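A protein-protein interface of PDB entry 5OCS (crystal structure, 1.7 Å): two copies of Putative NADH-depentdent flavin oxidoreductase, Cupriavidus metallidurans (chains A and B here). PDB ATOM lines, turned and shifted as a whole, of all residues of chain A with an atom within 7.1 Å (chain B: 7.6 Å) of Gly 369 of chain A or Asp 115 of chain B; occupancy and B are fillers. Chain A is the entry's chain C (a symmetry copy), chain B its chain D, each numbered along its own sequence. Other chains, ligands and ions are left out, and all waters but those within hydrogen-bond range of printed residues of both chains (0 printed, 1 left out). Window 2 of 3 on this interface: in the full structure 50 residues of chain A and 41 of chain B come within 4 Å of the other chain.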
ATOM      1  N   LYS A 349      -7.060  16.568 -20.580  1.00  0.00           N
ATOM      2  CA  LYS A 349      -8.228  15.966 -19.929  1.00  0.00           C
ATOM      3  C   LYS A 349      -9.492  15.835 -20.805  1.00  0.00           C
ATOM      4  O   LYS A 349     -10.247  14.872 -20.660  1.00  0.00           O
ATOM      5  CB  LYS A 349      -8.579  16.717 -18.650  1.00  0.00           C
ATOM      6  CG  LYS A 349      -9.056  18.129 -18.916  1.00  0.00           C
ATOM      7  CD  LYS A 349      -8.923  18.978 -17.692  1.00  0.00           C
ATOM      8  CE  LYS A 349      -9.415  20.392 -17.957  1.00  0.00           C
ATOM      9  NZ  LYS A 349      -9.085  21.273 -16.797  1.00  0.00           N
ATOM     10  N   TRP A 352      -9.404  12.454 -22.245  1.00  0.00           N
ATOM     11  CA  TRP A 352      -9.300  11.234 -21.430  1.00  0.00           C
ATOM     12  C   TRP A 352     -10.395  10.174 -21.706  1.00  0.00           C
ATOM     13  O   TRP A 352     -10.101   8.978 -21.742  1.00  0.00           O
ATOM     14  CB  TRP A 352      -9.251  11.563 -19.946  1.00  0.00           C
ATOM     15  CG  TRP A 352      -8.055  12.274 -19.511  1.00  0.00           C
ATOM     16  CD1 TRP A 352      -6.869  12.436 -20.198  1.00  0.00           C
ATOM     17  CD2 TRP A 352      -7.862  12.914 -18.238  1.00  0.00           C
ATOM     18  NE1 TRP A 352      -5.970  13.137 -19.425  1.00  0.00           N
ATOM     19  CE2 TRP A 352      -6.550  13.450 -18.229  1.00  0.00           C
ATOM     20  CE3 TRP A 352      -8.689  13.122 -17.119  1.00  0.00           C
ATOM     21  CZ2 TRP A 352      -6.043  14.168 -17.155  1.00  0.00           C
ATOM     22  CZ3 TRP A 352      -8.160  13.837 -16.030  1.00  0.00           C
ATOM     23  CH2 TRP A 352      -6.867  14.346 -16.065  1.00  0.00           C
ATOM     24  N   HIS A 367      -8.394  10.774 -14.349  1.00  0.00           N
ATOM     25  CA  HIS A 367      -9.276  10.384 -13.245  1.00  0.00           C
ATOM     26  C   HIS A 367     -10.657  10.987 -13.483  1.00  0.00           C
ATOM     27  O   HIS A 367     -10.816  11.985 -14.214  1.00  0.00           O
ATOM     28  CB  HIS A 367      -8.737  10.900 -11.923  1.00  0.00           C
ATOM     29  CG  HIS A 367      -8.686  12.384 -11.880  1.00  0.00           C
ATOM     30  ND1 HIS A 367      -7.674  13.103 -12.488  1.00  0.00           N
ATOM     31  CD2 HIS A 367      -9.593  13.294 -11.448  1.00  0.00           C
ATOM     32  CE1 HIS A 367      -7.931  14.397 -12.367  1.00  0.00           C
ATOM     33  NE2 HIS A 367      -9.091  14.536 -11.751  1.00  0.00           N
ATOM     34  N   PHE A 368     -11.635  10.405 -12.804  1.00  0.00           N
ATOM     35  CA  PHE A 368     -13.021  10.800 -12.948  1.00  0.00           C
ATOM     36  C   PHE A 368     -13.792  10.799 -11.615  1.00  0.00           C
ATOM     37  O   PHE A 368     -15.020  10.839 -11.637  1.00  0.00           O
ATOM     38  CB  PHE A 368     -13.678   9.867 -13.949  1.00  0.00           C
ATOM     39  CG  PHE A 368     -13.069   9.960 -15.309  1.00  0.00           C
ATOM     40  CD1 PHE A 368     -13.476  10.954 -16.186  1.00  0.00           C
ATOM     41  CD2 PHE A 368     -12.045   9.116 -15.686  1.00  0.00           C
ATOM     42  CE1 PHE A 368     -12.880  11.079 -17.434  1.00  0.00           C
ATOM     43  CE2 PHE A 368     -11.447   9.235 -16.938  1.00  0.00           C
ATOM     44  CZ  PHE A 368     -11.870  10.221 -17.809  1.00  0.00           C
ATOM     45  N   GLY A 369     -13.099  10.800 -10.479  1.00  0.00           N
ATOM     46  CA  GLY A 369     -13.767  10.760  -9.145  1.00  0.00           C
ATOM     47  C   GLY A 369     -14.206  12.117  -8.628  1.00  0.00           C
ATOM     48  O   GLY A 369     -13.589  13.129  -8.953  1.00  0.00           O
ATOM     49  N   TYR B  27     -16.389  20.935 -22.072  1.00  0.00           N
ATOM     50  CA  TYR B  27     -16.297  21.480 -20.691  1.00  0.00           C
ATOM     51  C   TYR B  27     -15.117  22.436 -20.551  1.00  0.00           C
ATOM     52  O   TYR B  27     -14.438  22.437 -19.547  1.00  0.00           O
ATOM     53  CB  TYR B  27     -16.176  20.321 -19.658  1.00  0.00           C
ATOM     54  CG  TYR B  27     -17.150  19.208 -19.905  1.00  0.00           C
ATOM     55  CD1 TYR B  27     -18.456  19.291 -19.418  1.00  0.00           C
ATOM     56  CD2 TYR B  27     -16.771  18.054 -20.604  1.00  0.00           C
ATOM     57  CE1 TYR B  27     -19.390  18.277 -19.679  1.00  0.00           C
ATOM     58  CE2 TYR B  27     -17.685  17.027 -20.851  1.00  0.00           C
ATOM     59  CZ  TYR B  27     -18.992  17.158 -20.370  1.00  0.00           C
ATOM     60  OH  TYR B  27     -19.915  16.169 -20.606  1.00  0.00           O
ATOM     61  N   THR B  69     -18.535  25.006 -17.126  1.00  0.00           N
ATOM     62  CA  THR B  69     -17.624  25.247 -18.241  1.00  0.00           C
ATOM     63  C   THR B  69     -18.187  24.787 -19.597  1.00  0.00           C
ATOM     64  O   THR B  69     -17.429  24.659 -20.551  1.00  0.00           O
ATOM     65  CB  THR B  69     -16.251  24.650 -17.960  1.00  0.00           C
ATOM     66  OG1 THR B  69     -16.353  23.288 -17.594  1.00  0.00           O
ATOM     67  CG2 THR B  69     -15.548  25.379 -16.828  1.00  0.00           C
ATOM     68  N   SER B 110     -23.979  20.777 -13.013  1.00  0.00           N
ATOM     69  CA  SER B 110     -23.204  19.582 -12.677  1.00  0.00           C
ATOM     70  C   SER B 110     -21.703  19.795 -12.959  1.00  0.00           C
ATOM     71  O   SER B 110     -21.291  20.748 -13.621  1.00  0.00           O
ATOM     72  CB  SER B 110     -23.689  18.397 -13.474  1.00  0.00           C
ATOM     73  OG  SER B 110     -25.037  18.111 -13.146  1.00  0.00           O
ATOM     74  N   GLU B 111     -20.896  18.896 -12.418  1.00  0.00           N
ATOM     75  CA  GLU B 111     -19.440  18.948 -12.582  1.00  0.00           C
ATOM     76  C   GLU B 111     -19.078  18.300 -13.903  1.00  0.00           C
ATOM     77  O   GLU B 111     -19.827  17.463 -14.420  1.00  0.00           O
ATOM     78  CB  GLU B 111     -18.734  18.187 -11.441  1.00  0.00           C
ATOM     79  CG  GLU B 111     -18.929  18.783 -10.058  1.00  0.00           C
ATOM     80  CD  GLU B 111     -18.137  20.075  -9.803  1.00  0.00           C
ATOM     81  OE1 GLU B 111     -17.601  20.722 -10.730  1.00  0.00           O
ATOM     82  OE2 GLU B 111     -18.093  20.524  -8.650  1.00  0.00           O
ATOM     83  N   ALA B 112     -17.936  18.697 -14.447  1.00  0.00           N
ATOM     84  CA  ALA B 112     -17.341  18.054 -15.609  1.00  0.00           C
ATOM     85  C   ALA B 112     -16.886  16.620 -15.281  1.00  0.00           C
ATOM     86  O   ALA B 112     -16.769  16.256 -14.093  1.00  0.00           O
ATOM     87  CB  ALA B 112     -16.186  18.913 -16.125  1.00  0.00           C
ATOM     88  N   PRO B 113     -16.689  15.763 -16.314  1.00  0.00           N
ATOM     89  CA  PRO B 113     -16.396  14.323 -16.036  1.00  0.00           C
ATOM     90  C   PRO B 113     -15.180  14.117 -15.139  1.00  0.00           C
ATOM     91  O   PRO B 113     -15.224  13.322 -14.206  1.00  0.00           O
ATOM     92  CB  PRO B 113     -16.143  13.747 -17.435  1.00  0.00           C
ATOM     93  CG  PRO B 113     -16.961  14.623 -18.354  1.00  0.00           C
ATOM     94  CD  PRO B 113     -16.898  16.008 -17.754  1.00  0.00           C
ATOM     95  N   TRP B 114     -14.100  14.839 -15.415  1.00  0.00           N
ATOM     96  CA  TRP B 114     -12.873  14.727 -14.602  1.00  0.00           C
ATOM     97  C   TRP B 114     -13.049  15.219 -13.164  1.00  0.00           C
ATOM     98  O   TRP B 114     -12.222  14.885 -12.308  1.00  0.00           O
ATOM     99  CB  TRP B 114     -11.658  15.414 -15.242  1.00  0.00           C
ATOM    100  CG  TRP B 114     -11.936  16.772 -15.831  1.00  0.00           C
ATOM    101  CD1 TRP B 114     -11.890  17.993 -15.207  1.00  0.00           C
ATOM    102  CD2 TRP B 114     -12.316  17.030 -17.182  1.00  0.00           C
ATOM    103  NE1 TRP B 114     -12.247  18.978 -16.081  1.00  0.00           N
ATOM    104  CE2 TRP B 114     -12.510  18.416 -17.303  1.00  0.00           C
ATOM    105  CE3 TRP B 114     -12.563  16.211 -18.298  1.00  0.00           C
ATOM    106  CZ2 TRP B 114     -12.888  19.012 -18.516  1.00  0.00           C
ATOM    107  CZ3 TRP B 114     -12.937  16.786 -19.474  1.00  0.00           C
ATOM    108  CH2 TRP B 114     -13.079  18.183 -19.590  1.00  0.00           C
ATOM    109  N   ASP B 115     -14.107  15.978 -12.897  1.00  0.00           N
ATOM    110  CA  ASP B 115     -14.462  16.387 -11.539  1.00  0.00           C
ATOM    111  C   ASP B 115     -15.574  15.544 -10.919  1.00  0.00           C
ATOM    112  O   ASP B 115     -16.101  15.913  -9.877  1.00  0.00           O
ATOM    113  CB  ASP B 115     -14.827  17.865 -11.537  1.00  0.00           C
ATOM    114  CG  ASP B 115     -13.657  18.754 -11.933  1.00  0.00           C
ATOM    115  OD1 ASP B 115     -12.511  18.421 -11.569  1.00  0.00           O
ATOM    116  OD2 ASP B 115     -13.895  19.747 -12.625  1.00  0.00           O
ATOM    117  N   GLY B 116     -15.907  14.420 -11.551  1.00  0.00           N
ATOM    118  CA  GLY B 116     -16.837  13.427 -10.975  1.00  0.00           C
ATOM    119  C   GLY B 116     -18.273  13.506 -11.435  1.00  0.00           C
ATOM    120  O   GLY B 116     -19.071  12.644 -11.085  1.00  0.00           O
ATOM    121  N   GLY B 117     -18.611  14.540 -12.206  1.00  0.00           N
ATOM    122  CA  GLY B 117     -19.919  14.636 -12.811  1.00  0.00           C
ATOM    123  C   GLY B 117     -21.099  14.875 -11.882  1.00  0.00           C
ATOM    124  O   GLY B 117     -22.255  14.823 -12.339  1.00  0.00           O
ATOM    125  N   GLY B 118     -20.827  15.164 -10.606  1.00  0.00           N
ATOM    126  CA  GLY B 118     -21.895  15.323  -9.597  1.00  0.00           C
ATOM    127  C   GLY B 118     -22.652  16.624  -9.699  1.00  0.00           C
ATOM    128  O   GLY B 118     -22.205  17.567 -10.348  1.00  0.00           O
ATOM    129  N   ARG B 126     -20.423  28.104  -7.748  1.00  0.00           N
ATOM    130  CA  ARG B 126     -20.656  27.722  -9.156  1.00  0.00           C
ATOM    131  C   ARG B 126     -22.005  27.075  -9.449  1.00  0.00           C
ATOM    132  O   ARG B 126     -22.335  26.948 -10.606  1.00  0.00           O
ATOM    133  CB  ARG B 126     -19.510  26.835  -9.720  1.00  0.00           C
ATOM    134  CG  ARG B 126     -18.110  27.473  -9.619  1.00  0.00           C
ATOM    135  CD  ARG B 126     -16.983  26.495  -9.983  1.00  0.00           C
ATOM    136  NE  ARG B 126     -17.058  25.377  -9.059  1.00  0.00           N
ATOM    137  CZ  ARG B 126     -17.304  24.098  -9.359  1.00  0.00           C
ATOM    138  NH1 ARG B 126     -17.406  23.660 -10.607  1.00  0.00           N
ATOM    139  NH2 ARG B 126     -17.425  23.233  -8.368  1.00  0.00           N
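NE2 of His 367 of chain A lies close to O of Trp 114 of chain B (3.2 Å).
Among the printed residues, pairs that only touch across the chains: Lys 349 of chain A with Trp 114 of chain B (3.5 Å), Trp 352 of chain A with Trp 114 of chain B (3.9 Å), Phe 368 of chain A with Pro 113 of chain B (3.5 Å), Phe 368 of chain A with Gly 116 of chain B (3.2 Å), Gly 369 of chain A with Asp 115 of chain B (3.7 Å) and Gly 369 of chain A with Gly 116 of chain B (3.7 Å).
Printed residues of chain B within 4 Å of Gly 369 of chain A: Asp 115 (3.7 Å) and Gly 116 (3.7 Å). Of chain A, only Gly 369 (3.7 Å) comes within 4 Å of Asp 115 of chain B. Printed residues of chain A within 4 Å of Pro 113 of chain B: Phe 368. Printed residues of chain B within 4 Å of His 367 of chain A: Trp 114. Printed residues of chain B within 4 Å of Trp 352 of chain A: Trp 114 (3.9 Å). Of the printed residues of chain B, Phe 368 of chain A touches Pro 113 (3.5 Å) and Gly 116 (3.2 Å). The nearest residue of chain B that does not touch Gly 369 of chain A is Trp 114 of chain B (4.03 Å). The nearest printed residue of chain A that does not touch Trp 114 of chain B is Phe 368 of chain A (4.01 Å).
Of the 5 printed residues of chain A, 5 touch a printed residue of chain B. Hydrophobic or aromatic side chains of chain A that line the printed part of chain B: Trp 352, His 367 and Phe 368. Hydrophobic or aromatic side chains of chain B within 4 Å of the printed part of chain A: Trp 114. Along chain B the printed residues that touch a printed residue of chain A span positions 113 to 116. Among the printed residues, no Asp or Glu carboxylate lies within 4 Å of a Lys or Arg side-chain nitrogen of the other chain.
No position is printed for both chains. Of the 7 pairs that touch across the chains among the printed residues, none has its exchanged pair printed and touching as well.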
